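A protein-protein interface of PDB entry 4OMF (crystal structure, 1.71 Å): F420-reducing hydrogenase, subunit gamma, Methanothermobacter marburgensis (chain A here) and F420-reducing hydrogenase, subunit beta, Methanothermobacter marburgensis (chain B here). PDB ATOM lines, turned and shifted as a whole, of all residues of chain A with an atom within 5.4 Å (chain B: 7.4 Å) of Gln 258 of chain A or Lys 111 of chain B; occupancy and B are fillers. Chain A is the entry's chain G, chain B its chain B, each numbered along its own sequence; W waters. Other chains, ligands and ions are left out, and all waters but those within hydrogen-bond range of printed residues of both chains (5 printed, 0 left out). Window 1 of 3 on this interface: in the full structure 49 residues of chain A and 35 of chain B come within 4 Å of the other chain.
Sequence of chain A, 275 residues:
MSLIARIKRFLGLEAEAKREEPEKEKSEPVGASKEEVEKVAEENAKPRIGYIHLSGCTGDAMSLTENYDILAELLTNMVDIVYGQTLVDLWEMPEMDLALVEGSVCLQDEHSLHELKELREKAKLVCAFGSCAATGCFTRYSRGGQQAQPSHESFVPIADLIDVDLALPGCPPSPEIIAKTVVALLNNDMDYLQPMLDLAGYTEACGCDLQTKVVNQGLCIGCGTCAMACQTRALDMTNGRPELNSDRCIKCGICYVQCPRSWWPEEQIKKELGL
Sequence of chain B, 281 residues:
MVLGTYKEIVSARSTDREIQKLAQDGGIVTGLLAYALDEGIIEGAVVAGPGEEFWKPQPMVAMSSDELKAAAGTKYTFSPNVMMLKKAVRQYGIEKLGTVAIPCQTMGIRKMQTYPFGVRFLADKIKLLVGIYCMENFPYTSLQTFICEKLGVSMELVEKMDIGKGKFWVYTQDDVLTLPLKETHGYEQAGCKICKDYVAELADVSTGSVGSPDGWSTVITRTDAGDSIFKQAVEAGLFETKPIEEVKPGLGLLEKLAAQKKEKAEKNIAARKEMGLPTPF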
ATOM      1  N   THR A 225     -23.567  -4.961 -18.060  1.00  0.00           N
ATOM      2  CA  THR A 225     -23.657  -3.503 -18.213  1.00  0.00           C
ATOM      3  C   THR A 225     -22.758  -3.032 -19.365  1.00  0.00           C
ATOM      4  O   THR A 225     -23.121  -2.157 -20.167  1.00  0.00           O
ATOM      5  CB  THR A 225     -23.277  -2.782 -16.894  1.00  0.00           C
ATOM      6  OG1 THR A 225     -24.149  -3.207 -15.836  1.00  0.00           O
ATOM      7  CG2 THR A 225     -23.363  -1.270 -17.053  1.00  0.00           C
ATOM      8  N   ALA A 229     -23.926  -0.968 -22.833  1.00  0.00           N
ATOM      9  CA  ALA A 229     -23.448   0.382 -23.083  1.00  0.00           C
ATOM     10  C   ALA A 229     -22.793   0.554 -24.448  1.00  0.00           C
ATOM     11  O   ALA A 229     -22.951   1.605 -25.071  1.00  0.00           O
ATOM     12  CB  ALA A 229     -22.474   0.791 -21.997  1.00  0.00           C
ATOM     13  N   GLY A 253     -13.577   3.266 -24.845  1.00  0.00           N
ATOM     14  CA  GLY A 253     -13.543   3.125 -23.394  1.00  0.00           C
ATOM     15  C   GLY A 253     -14.867   3.060 -22.640  1.00  0.00           C
ATOM     16  O   GLY A 253     -14.869   2.886 -21.422  1.00  0.00           O
ATOM     17  N   ILE A 254     -15.994   3.171 -23.341  1.00  0.00           N
ATOM     18  CA  ILE A 254     -17.296   3.316 -22.680  1.00  0.00           C
ATOM     19  C   ILE A 254     -17.682   2.061 -21.852  1.00  0.00           C
ATOM     20  O   ILE A 254     -18.279   2.196 -20.778  1.00  0.00           O
ATOM     21  CB  ILE A 254     -18.397   3.644 -23.715  1.00  0.00           C
ATOM     22  CG1 ILE A 254     -18.410   5.153 -24.013  1.00  0.00           C
ATOM     23  CG2 ILE A 254     -19.796   3.223 -23.229  1.00  0.00           C
ATOM     24  CD1 ILE A 254     -18.599   5.997 -22.758  1.00  0.00           C
ATOM     25  N   CYS A 255     -17.318   0.869 -22.321  1.00  0.00           N
ATOM     26  CA  CYS A 255     -17.672  -0.354 -21.610  1.00  0.00           C
ATOM     27  C   CYS A 255     -17.054  -0.345 -20.203  1.00  0.00           C
ATOM     28  O   CYS A 255     -17.724  -0.655 -19.229  1.00  0.00           O
ATOM     29  CB  CYS A 255     -17.220  -1.594 -22.404  1.00  0.00           C
ATOM     30  SG  CYS A 255     -15.509  -1.506 -22.975  1.00  0.00           S
ATOM     31  N   TYR A 256     -15.782   0.015 -20.125  1.00  0.00           N
ATOM     32  CA  TYR A 256     -15.101   0.076 -18.842  1.00  0.00           C
ATOM     33  C   TYR A 256     -15.586   1.272 -17.999  1.00  0.00           C
ATOM     34  O   TYR A 256     -15.696   1.178 -16.771  1.00  0.00           O
ATOM     35  CB  TYR A 256     -13.582   0.111 -19.058  1.00  0.00           C
ATOM     36  CG  TYR A 256     -12.820   0.122 -17.759  1.00  0.00           C
ATOM     37  CD1 TYR A 256     -12.129   1.259 -17.353  1.00  0.00           C
ATOM     38  CD2 TYR A 256     -12.831  -0.986 -16.905  1.00  0.00           C
ATOM     39  CE1 TYR A 256     -11.443   1.294 -16.149  1.00  0.00           C
ATOM     40  CE2 TYR A 256     -12.152  -0.957 -15.703  1.00  0.00           C
ATOM     41  CZ  TYR A 256     -11.459   0.188 -15.327  1.00  0.00           C
ATOM     42  OH  TYR A 256     -10.775   0.255 -14.130  1.00  0.00           O
ATOM     43  N   VAL A 257     -15.920   2.371 -18.665  1.00  0.00           N
ATOM     44  CA  VAL A 257     -16.490   3.526 -17.983  1.00  0.00           C
ATOM     45  C   VAL A 257     -17.783   3.157 -17.257  1.00  0.00           C
ATOM     46  O   VAL A 257     -17.962   3.506 -16.087  1.00  0.00           O
ATOM     47  CB  VAL A 257     -16.749   4.701 -18.969  1.00  0.00           C
ATOM     48  CG1 VAL A 257     -17.538   5.819 -18.260  1.00  0.00           C
ATOM     49  CG2 VAL A 257     -15.411   5.250 -19.458  1.00  0.00           C
ATOM     50  N   GLN A 258     -18.655   2.398 -17.921  1.00  0.00           N
ATOM     51  CA  GLN A 258     -19.980   2.095 -17.343  1.00  0.00           C
ATOM     52  C   GLN A 258     -19.975   0.889 -16.396  1.00  0.00           C
ATOM     53  O   GLN A 258     -20.825   0.808 -15.522  1.00  0.00           O
ATOM     54  CB  GLN A 258     -21.014   1.860 -18.450  1.00  0.00           C
ATOM     55  CG  GLN A 258     -21.150   3.002 -19.473  1.00  0.00           C
ATOM     56  CD  GLN A 258     -21.782   4.291 -18.948  1.00  0.00           C
ATOM     57  OE1 GLN A 258     -21.705   5.306 -19.624  1.00  0.00           O
ATOM     58  NE2 GLN A 258     -22.415   4.262 -17.749  1.00  0.00           N
ATOM     59  N   CYS A 259     -19.024  -0.031 -16.571  1.00  0.00           N
ATOM     60  CA  CYS A 259     -18.849  -1.145 -15.630  1.00  0.00           C
ATOM     61  C   CYS A 259     -18.980  -0.696 -14.160  1.00  0.00           C
ATOM     62  O   CYS A 259     -18.279   0.217 -13.722  1.00  0.00           O
ATOM     63  CB  CYS A 259     -17.477  -1.787 -15.865  1.00  0.00           C
ATOM     64  SG  CYS A 259     -17.081  -3.124 -14.725  1.00  0.00           S
ATOM     65  N   PRO A 260     -19.877  -1.337 -13.393  1.00  0.00           N
ATOM     66  CA  PRO A 260     -20.042  -0.952 -11.994  1.00  0.00           C
ATOM     67  C   PRO A 260     -18.804  -1.290 -11.165  1.00  0.00           C
ATOM     68  O   PRO A 260     -18.679  -0.836 -10.038  1.00  0.00           O
ATOM     69  CB  PRO A 260     -21.247  -1.783 -11.544  1.00  0.00           C
ATOM     70  CG  PRO A 260     -21.185  -3.037 -12.445  1.00  0.00           C
ATOM     71  CD  PRO A 260     -20.736  -2.484 -13.767  1.00  0.00           C
ATOM     72  N   ARG A 261     -17.899  -2.078 -11.719  1.00  0.00           N
ATOM     73  CA  ARG A 261     -16.742  -2.486 -10.920  1.00  0.00           C
ATOM     74  C   ARG A 261     -15.477  -1.680 -11.266  1.00  0.00           C
ATOM     75  O   ARG A 261     -14.420  -1.912 -10.683  1.00  0.00           O
ATOM     76  CB  ARG A 261     -16.489  -4.010 -11.082  1.00  0.00           C
ATOM     77  CG  ARG A 261     -17.554  -4.872 -10.434  1.00  0.00           C
ATOM     78  CD  ARG A 261     -17.260  -4.987  -8.951  1.00  0.00           C
ATOM     79  NE  ARG A 261     -18.254  -5.700  -8.153  1.00  0.00           N
ATOM     80  CZ  ARG A 261     -18.064  -6.911  -7.631  1.00  0.00           C
ATOM     81  NH1 ARG A 261     -16.948  -7.601  -7.885  1.00  0.00           N
ATOM     82  NH2 ARG A 261     -18.989  -7.431  -6.847  1.00  0.00           N
ATOM     83  N   SER A 262     -15.581  -0.721 -12.186  1.00  0.00           N
ATOM     84  CA  SER A 262     -14.441   0.162 -12.477  1.00  0.00           C
ATOM     85  C   SER A 262     -14.322   1.308 -11.450  1.00  0.00           C
ATOM     86  O   SER A 262     -13.247   1.609 -10.952  1.00  0.00           O
ATOM     87  CB  SER A 262     -14.550   0.738 -13.885  1.00  0.00           C
ATOM     88  OG  SER A 262     -15.747   1.484 -14.020  1.00  0.00           O
ATOM     89  N   TRP A 263     -15.440   1.942 -11.151  1.00  0.00           N
ATOM     90  CA  TRP A 263     -15.496   2.956 -10.112  1.00  0.00           C
ATOM     91  C   TRP A 263     -16.958   3.010  -9.704  1.00  0.00           C
ATOM     92  O   TRP A 263     -17.858   2.792 -10.528  1.00  0.00           O
ATOM     93  CB  TRP A 263     -14.968   4.319 -10.594  1.00  0.00           C
ATOM     94  CG  TRP A 263     -15.496   4.771 -11.943  1.00  0.00           C
ATOM     95  CD1 TRP A 263     -14.969   4.464 -13.175  1.00  0.00           C
ATOM     96  CD2 TRP A 263     -16.617   5.645 -12.194  1.00  0.00           C
ATOM     97  NE1 TRP A 263     -15.714   5.077 -14.171  1.00  0.00           N
ATOM     98  CE2 TRP A 263     -16.713   5.819 -13.594  1.00  0.00           C
ATOM     99  CE3 TRP A 263     -17.532   6.309 -11.369  1.00  0.00           C
ATOM    100  CZ2 TRP A 263     -17.728   6.602 -14.194  1.00  0.00           C
ATOM    101  CZ3 TRP A 263     -18.534   7.094 -11.960  1.00  0.00           C
ATOM    102  CH2 TRP A 263     -18.618   7.237 -13.359  1.00  0.00           C
ATOM    103  N   TRP A 264     -17.191   3.275  -8.431  1.00  0.00           N
ATOM    104  CA  TRP A 264     -18.526   3.130  -7.891  1.00  0.00           C
ATOM    105  C   TRP A 264     -18.952   4.406  -7.150  1.00  0.00           C
ATOM    106  O   TRP A 264     -18.603   4.618  -5.983  1.00  0.00           O
ATOM    107  CB  TRP A 264     -18.586   1.888  -6.981  1.00  0.00           C
ATOM    108  CG  TRP A 264     -19.897   1.759  -6.292  1.00  0.00           C
ATOM    109  CD1 TRP A 264     -20.131   1.780  -4.940  1.00  0.00           C
ATOM    110  CD2 TRP A 264     -21.171   1.635  -6.921  1.00  0.00           C
ATOM    111  NE1 TRP A 264     -21.478   1.654  -4.695  1.00  0.00           N
ATOM    112  CE2 TRP A 264     -22.138   1.563  -5.895  1.00  0.00           C
ATOM    113  CE3 TRP A 264     -21.586   1.541  -8.243  1.00  0.00           C
ATOM    114  CZ2 TRP A 264     -23.501   1.439  -6.160  1.00  0.00           C
ATOM    115  CZ3 TRP A 264     -22.950   1.423  -8.507  1.00  0.00           C
ATOM    116  CH2 TRP A 264     -23.885   1.376  -7.466  1.00  0.00           C
ATOM    117  N   PRO A 265     -19.733   5.261  -7.829  1.00  0.00           N
ATOM    118  CA  PRO A 265     -20.053   6.567  -7.262  1.00  0.00           C
ATOM    119  C   PRO A 265     -21.277   6.471  -6.348  1.00  0.00           C
ATOM    120  O   PRO A 265     -22.351   6.982  -6.658  1.00  0.00           O
ATOM    121  CB  PRO A 265     -20.328   7.415  -8.507  1.00  0.00           C
ATOM    122  CG  PRO A 265     -20.990   6.434  -9.451  1.00  0.00           C
ATOM    123  CD  PRO A 265     -20.262   5.100  -9.197  1.00  0.00           C
ATOM    124  N   ILE A 269     -25.079   8.352  -6.617  1.00  0.00           N
ATOM    125  CA  ILE A 269     -26.176   7.495  -7.049  1.00  0.00           C
ATOM    126  C   ILE A 269     -27.340   7.555  -6.052  1.00  0.00           C
ATOM    127  O   ILE A 269     -28.488   7.745  -6.446  1.00  0.00           O
ATOM    128  CB  ILE A 269     -25.696   6.046  -7.248  1.00  0.00           C
ATOM    129  CG1 ILE A 269     -24.938   5.936  -8.580  1.00  0.00           C
ATOM    130  CG2 ILE A 269     -26.866   5.051  -7.115  1.00  0.00           C
ATOM    131  CD1 ILE A 269     -24.274   4.584  -8.797  1.00  0.00           C
ATOM    132  N   GLN B 105     -26.403  -6.110 -10.698  1.00  0.00           N
ATOM    133  CA  GLN B 105     -27.019  -5.590 -11.916  1.00  0.00           C
ATOM    134  C   GLN B 105     -27.717  -4.276 -11.635  1.00  0.00           C
ATOM    135  O   GLN B 105     -27.646  -3.351 -12.450  1.00  0.00           O
ATOM    136  CB  GLN B 105     -27.996  -6.596 -12.511  1.00  0.00           C
ATOM    137  CG  GLN B 105     -27.277  -7.785 -13.164  1.00  0.00           C
ATOM    138  CD  GLN B 105     -28.220  -8.918 -13.497  1.00  0.00           C
ATOM    139  OE1 GLN B 105     -29.439  -8.819 -13.293  1.00  0.00           O
ATOM    140  NE2 GLN B 105     -27.661 -10.025 -13.960  1.00  0.00           N
ATOM    141  N   THR B 106     -28.380  -4.175 -10.484  1.00  0.00           N
ATOM    142  CA  THR B 106     -29.010  -2.928 -10.088  1.00  0.00           C
ATOM    143  C   THR B 106     -27.951  -1.816 -10.046  1.00  0.00           C
ATOM    144  O   THR B 106     -28.218  -0.686 -10.408  1.00  0.00           O
ATOM    145  CB  THR B 106     -29.719  -3.095  -8.729  1.00  0.00           C
ATOM    146  OG1 THR B 106     -30.716  -4.121  -8.848  1.00  0.00           O
ATOM    147  CG2 THR B 106     -30.395  -1.820  -8.286  1.00  0.00           C
ATOM    148  N   MET B 107     -26.738  -2.152  -9.605  1.00  0.00           N
ATOM    149  CA  MET B 107     -25.673  -1.150  -9.533  1.00  0.00           C
ATOM    150  C   MET B 107     -25.230  -0.628 -10.903  1.00  0.00           C
ATOM    151  O   MET B 107     -25.044   0.572 -11.093  1.00  0.00           O
ATOM    152  CB  MET B 107     -24.468  -1.719  -8.788  1.00  0.00           C
ATOM    153  CG  MET B 107     -24.806  -2.010  -7.345  1.00  0.00           C
ATOM    154  SD  MET B 107     -23.434  -2.834  -6.494  1.00  0.00           S
ATOM    155  CE  MET B 107     -24.327  -3.809  -5.312  1.00  0.00           C
ATOM    156  N   GLY B 108     -25.045  -1.525 -11.856  1.00  0.00           N
ATOM    157  CA  GLY B 108     -24.717  -1.104 -13.197  1.00  0.00           C
ATOM    158  C   GLY B 108     -25.791  -0.208 -13.776  1.00  0.00           C
ATOM    159  O   GLY B 108     -25.482   0.780 -14.440  1.00  0.00           O
ATOM    160  N   ILE B 109     -27.061  -0.558 -13.544  1.00  0.00           N
ATOM    161  CA  ILE B 109     -28.174   0.258 -14.036  1.00  0.00           C
ATOM    162  C   ILE B 109     -28.206   1.660 -13.396  1.00  0.00           C
ATOM    163  O   ILE B 109     -28.377   2.652 -14.089  1.00  0.00           O
ATOM    164  CB  ILE B 109     -29.546  -0.460 -13.793  1.00  0.00           C
ATOM    165  CG1 ILE B 109     -29.610  -1.759 -14.613  1.00  0.00           C
ATOM    166  CG2 ILE B 109     -30.739   0.481 -14.079  1.00  0.00           C
ATOM    167  CD1 ILE B 109     -30.754  -2.670 -14.206  1.00  0.00           C
ATOM    168  N   ARG B 110     -28.054   1.736 -12.079  1.00  0.00           N
ATOM    169  CA  ARG B 110     -28.153   3.018 -11.381  1.00  0.00           C
ATOM    170  C   ARG B 110     -26.940   3.879 -11.740  1.00  0.00           C
ATOM    171  O   ARG B 110     -27.045   5.106 -11.854  1.00  0.00           O
ATOM    172  CB  ARG B 110     -28.248   2.822  -9.855  1.00  0.00           C
ATOM    173  CG  ARG B 110     -29.524   2.138  -9.359  1.00  0.00           C
ATOM    174  CD  ARG B 110     -30.791   2.770  -9.917  1.00  0.00           C
ATOM    175  NE  ARG B 110     -31.956   2.395  -9.117  1.00  0.00           N
ATOM    176  CZ  ARG B 110     -33.212   2.615  -9.487  1.00  0.00           C
ATOM    177  NH1 ARG B 110     -34.215   2.234  -8.706  1.00  0.00           N
ATOM    178  NH2 ARG B 110     -33.469   3.191 -10.655  1.00  0.00           N
ATOM    179  N   LYS B 111     -25.791   3.231 -11.922  1.00  0.00           N
ATOM    180  CA  LYS B 111     -24.599   3.955 -12.344  1.00  0.00           C
ATOM    181  C   LYS B 111     -24.833   4.550 -13.724  1.00  0.00           C
ATOM    182  O   LYS B 111     -24.447   5.685 -13.985  1.00  0.00           O
ATOM    183  CB  LYS B 111     -23.351   3.046 -12.370  1.00  0.00           C
ATOM    184  CG  LYS B 111     -22.080   3.780 -12.837  1.00  0.00           C
ATOM    185  CD  LYS B 111     -20.842   2.916 -12.713  1.00  0.00           C
ATOM    186  CE  LYS B 111     -19.674   3.599 -13.410  1.00  0.00           C
ATOM    187  NZ  LYS B 111     -18.388   2.790 -13.330  1.00  0.00           N
ATOM    188  N   MET B 112     -25.489   3.789 -14.599  1.00  0.00           N
ATOM    189  CA  MET B 112     -25.776   4.286 -15.936  1.00  0.00           C
ATOM    190  C   MET B 112     -26.707   5.489 -15.868  1.00  0.00           C
ATOM    191  O   MET B 112     -26.499   6.473 -16.585  1.00  0.00           O
ATOM    192  CB  MET B 112     -26.395   3.181 -16.815  1.00  0.00           C
ATOM    193  CG  MET B 112     -26.951   3.679 -18.158  1.00  0.00           C
ATOM    194  SD  MET B 112     -28.705   4.163 -18.094  1.00  0.00           S
ATOM    195  CE  MET B 112     -29.484   2.580 -17.668  1.00  0.00           C
ATOM    196  N   GLN B 113     -27.706   5.441 -14.977  1.00  0.00           N
ATOM    197  CA  GLN B 113     -28.703   6.517 -14.961  1.00  0.00           C
ATOM    198  C   GLN B 113     -28.080   7.818 -14.454  1.00  0.00           C
ATOM    199  O   GLN B 113     -28.386   8.906 -14.941  1.00  0.00           O
ATOM    200  CB  GLN B 113     -29.907   6.161 -14.088  1.00  0.00           C
ATOM    201  CG  GLN B 113     -30.792   5.022 -14.609  1.00  0.00           C
ATOM    202  CD  GLN B 113     -31.964   4.745 -13.669  1.00  0.00           C
ATOM    203  OE1 GLN B 113     -31.765   4.360 -12.512  1.00  0.00           O
ATOM    204  NE2 GLN B 113     -33.179   4.974 -14.142  1.00  0.00           N
ATOM    205  N   THR B 114     -27.190   7.693 -13.476  1.00  0.00           N
ATOM    206  CA  THR B 114     -26.558   8.861 -12.881  1.00  0.00           C
ATOM    207  C   THR B 114     -25.432   9.382 -13.770  1.00  0.00           C
ATOM    208  O   THR B 114     -25.246  10.605 -13.875  1.00  0.00           O
ATOM    209  CB  THR B 114     -26.026   8.524 -11.479  1.00  0.00           C
ATOM    210  OG1 THR B 114     -27.138   8.161 -10.658  1.00  0.00           O
ATOM    211  CG2 THR B 114     -25.367   9.730 -10.831  1.00  0.00           C
ATOM    212  N   TYR B 115     -24.702   8.456 -14.398  1.00  0.00           N
ATOM    213  CA  TYR B 115     -23.594   8.777 -15.313  1.00  0.00           C
ATOM    214  C   TYR B 115     -23.695   8.082 -16.673  1.00  0.00           C
ATOM    215  O   TYR B 115     -22.953   7.136 -16.946  1.00  0.00           O
ATOM    216  CB  TYR B 115     -22.251   8.384 -14.677  1.00  0.00           C
ATOM    217  CG  TYR B 115     -21.880   9.249 -13.497  1.00  0.00           C
ATOM    218  CD1 TYR B 115     -21.356  10.512 -13.690  1.00  0.00           C
ATOM    219  CD2 TYR B 115     -22.054   8.800 -12.186  1.00  0.00           C
ATOM    220  CE1 TYR B 115     -20.996  11.309 -12.612  1.00  0.00           C
ATOM    221  CE2 TYR B 115     -21.713   9.596 -11.103  1.00  0.00           C
ATOM    222  CZ  TYR B 115     -21.186  10.848 -11.326  1.00  0.00           C
ATOM    223  OH  TYR B 115     -20.830  11.669 -10.275  1.00  0.00           O
ATOM    224  N   PRO B 116     -24.596   8.563 -17.540  1.00  0.00           N
ATOM    225  CA  PRO B 116     -24.820   7.877 -18.822  1.00  0.00           C
ATOM    226  C   PRO B 116     -23.834   8.319 -19.902  1.00  0.00           C
ATOM    227  O   PRO B 116     -24.282   8.770 -20.957  1.00  0.00           O
ATOM    228  CB  PRO B 116     -26.242   8.294 -19.185  1.00  0.00           C
ATOM    229  CG  PRO B 116     -26.364   9.699 -18.578  1.00  0.00           C
ATOM    230  CD  PRO B 116     -25.652   9.559 -17.247  1.00  0.00           C
ATOM    231  N   PHE B 117     -22.536   8.185 -19.646  1.00  0.00           N
ATOM    232  CA  PHE B 117     -21.529   8.666 -20.586  1.00  0.00           C
ATOM    233  C   PHE B 117     -21.798   8.193 -22.004  1.00  0.00           C
ATOM    234  O   PHE B 117     -21.923   9.025 -22.902  1.00  0.00           O
ATOM    235  CB  PHE B 117     -20.127   8.223 -20.177  1.00  0.00           C
ATOM    236  CG  PHE B 117     -19.567   9.002 -19.048  1.00  0.00           C
ATOM    237  CD1 PHE B 117     -19.749   8.577 -17.729  1.00  0.00           C
ATOM    238  CD2 PHE B 117     -18.850  10.168 -19.295  1.00  0.00           C
ATOM    239  CE1 PHE B 117     -19.215   9.316 -16.683  1.00  0.00           C
ATOM    240  CE2 PHE B 117     -18.327  10.900 -18.258  1.00  0.00           C
ATOM    241  CZ  PHE B 117     -18.504  10.475 -16.958  1.00  0.00           C
ATOM    242  N   GLY B 118     -21.932   6.882 -22.194  1.00  0.00           N
ATOM    243  CA  GLY B 118     -22.101   6.356 -23.551  1.00  0.00           C
ATOM    244  C   GLY B 118     -23.517   5.869 -23.848  1.00  0.00           C
ATOM    245  O   GLY B 118     -23.737   5.136 -24.812  1.00  0.00           O
ATOM    246  N   VAL B 119     -24.475   6.252 -23.011  1.00  0.00           N
ATOM    247  CA  VAL B 119     -25.817   5.641 -23.079  1.00  0.00           C
ATOM    248  C   VAL B 119     -26.878   6.712 -23.357  1.00  0.00           C
ATOM    249  O   VAL B 119     -27.267   7.484 -22.473  1.00  0.00           O
ATOM    250  CB  VAL B 119     -26.142   4.866 -21.778  1.00  0.00           C
ATOM    251  CG1 VAL B 119     -27.458   4.106 -21.910  1.00  0.00           C
ATOM    252  CG2 VAL B 119     -25.004   3.868 -21.466  1.00  0.00           C
ATOM    253  N   LEU B 202     -30.576  -0.575  -3.910  1.00  0.00           N
ATOM    254  CA  LEU B 202     -30.802   0.561  -4.798  1.00  0.00           C
ATOM    255  C   LEU B 202     -32.004   0.360  -5.730  1.00  0.00           C
ATOM    256  O   LEU B 202     -32.268   1.191  -6.598  1.00  0.00           O
ATOM    257  CB  LEU B 202     -29.533   0.851  -5.623  1.00  0.00           C
ATOM    258  CG  LEU B 202     -28.311   1.217  -4.754  1.00  0.00           C
ATOM    259  CD1 LEU B 202     -27.034   1.433  -5.574  1.00  0.00           C
ATOM    260  CD2 LEU B 202     -28.604   2.436  -3.914  1.00  0.00           C
HETATM  261  O   HOH W   1     -23.127   2.102 -15.892  1.00  0.00           O
HETATM  262  O   HOH W   2     -20.848  -4.394  -8.149  1.00  0.00           O
HETATM  263  O   HOH W   3     -21.183  -5.757  -5.633  1.00  0.00           O
HETATM  264  O   HOH W   4     -29.051   6.582  -9.681  1.00  0.00           O
HETATM  265  O   HOH W   5     -20.427  -1.725  -8.105  1.00  0.00           O
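Water W4 lies within hydrogen-bond range of OG1 of Thr 114 of chain B (2.7 Å), O of Arg 110 of chain B (3.3 Å) and O of Ile 269 of chain A (3.5 Å). Water W1 lies within hydrogen-bond range of O of Gln 258 of chain A (2.7 Å), O of Gly 108 of chain B (3.1 Å) and N of Met 112 of chain B (3.2 Å). Water W5 lies within hydrogen-bond range of O of Pro 260 of chain A (2.8 Å) and SD of Met 107 of chain B (3.6 Å). Water W2 lies within hydrogen-bond range of NE of Arg 261 of chain A and SD of Met 107 of chain B. Water W3 bridges the guanidinium group of Arg 261 of chain A and the side-chain sulfur of Met 107 of chain B.
The backbone carbonyl oxygen (O) of Cys 259 of chain A lies within hydrogen-bond range of the side-chain amino group (NZ) of Lys 111 of chain B (2.6 Å). The backbone carbonyl oxygen of Val 257 of chain A sits at hydrogen-bond distance from the side-chain amino group of Lys 111 of chain B (2.9 Å). The side-chain hydroxyl of Ser 262 of chain A is in hydrogen-bond range of the side-chain amino group of Lys 111 of chain B, 3.0 Å away. OE1 of Gln 258 of chain A lies within hydrogen-bond range of N of Phe 117 of chain B. The backbone carbonyl oxygen of Trp 263 of chain A is in hydrogen-bond range of the side-chain amino group of Lys 111 of chain B (2.9 Å). O of Tyr 115 of chain B lies within hydrogen-bond range of NE2 of Gln 258 of chain A (3.0 Å). N of Gly 118 of chain B lies within hydrogen-bond range of OE1 of Gln 258 of chain A, at 3.0 Å.
Among the printed residues, merely in contact across the chains: Trp 264 of chain A with Met 107 of chain B, Thr 225 of chain A with Gly 108 of chain B, Ile 254 of chain A with Gly 118 of chain B, Gln 258 of chain A with Lys 111 of chain B, Val 257 of chain A with Phe 117 of chain B, Trp 264 of chain A with Leu 202 of chain B, Ile 269 of chain A with Lys 111 of chain B, Ala 229 of chain A with Gly 118 of chain B, Pro 265 of chain A with Tyr 115 of chain B, Gln 258 of chain A with Pro 116 of chain B, Ile 254 of chain A with Phe 117 of chain B, Ile 269 of chain A with Thr 114 of chain B, Ile 269 of chain A with Arg 110 of chain B, Gln 258 of chain A with Met 112 of chain B, Pro 260 of chain A with Gly 108 of chain B, Trp 263 of chain A with Tyr 115 of chain B, Ile 269 of chain A with Leu 202 of chain B and Trp 263 of chain A with Phe 117 of chain B.
SG of Cys 259 of chain A lies close to N of Arg 261 of chain A, at 3.3 Å. O of Cys 259 of chain A is in hydrogen-bond range of OG of Ser 262 of chain A (2.8 Å). The backbone carbonyl oxygen of Tyr 256 of chain A is in hydrogen-bond range of the side-chain hydroxyl of Ser 262 of chain A, at 2.8 Å. The guanidinium group (NH2) of Arg 110 of chain B sits at hydrogen-bond distance from the side-chain amide oxygen (OE1) of Gln 113 of chain B (2.8 Å). The backbone carbonyl oxygen (O) of Val 257 of chain A sits at hydrogen-bond distance from the indole nitrogen (NE1) of Trp 263 of chain A (3.3 Å). The backbone carbonyl oxygen of Leu 202 of chain B sits at hydrogen-bond distance from the guanidinium group of Arg 110 of chain B (2.8 Å).
Of the 16 printed residues of chain B, 11 touch a printed residue of chain A. Printed residues of chain B that touch a printed residue of chain A: Met 107, Gly 108, Arg 110, Lys 111, Met 112, Thr 114, Tyr 115, Pro 116, Phe 117, Gly 118 and Leu 202. Hydrophobic or aromatic side chains of chain B that line the printed part of chain A: Met 107, Tyr 115, Phe 117 and Leu 202. Of the 16 printed residues of chain A, 12 touch a printed residue of chain B. Hydrophobic or aromatic side chains of chain A that line the printed part of chain B: Ile 254, Val 257, Pro 260, Trp 263, Trp 264, Pro 265 and Ile 269. Among the printed residues, 25 pairs touch across the chains.
Of the printed residues of chain B, Gln 258 of chain A touches Lys 111 (3.5 Å), Met 112 (3.8 Å), Tyr 115 (3.0 Å), Pro 116 (3.7 Å), Phe 117 (3.0 Å) and Gly 118 (3.0 Å). Of the printed residues of chain A, Lys 111 of chain B touches Val 257 (2.9 Å), Gln 258 (3.5 Å), Cys 259 (2.6 Å), Ser 262 (3.0 Å), Trp 263 (2.9 Å) and Ile 269 (3.6 Å). Of the printed residues of chain A, Pro 116 of chain B touches Gln 258. Printed residues of chain B within 4 Å of Cys 259 of chain A: Lys 111 (2.6 Å). Printed residues of chain B within 4 Å of Val 257 of chain A: Lys 111 (2.9 Å) and Phe 117 (3.6 Å). Thr 106 of chain B touches none of the printed residues of chain A. The nearest residue of chain B that does not touch Gln 258 of chain A is Val 119 of chain B (4.04 Å).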
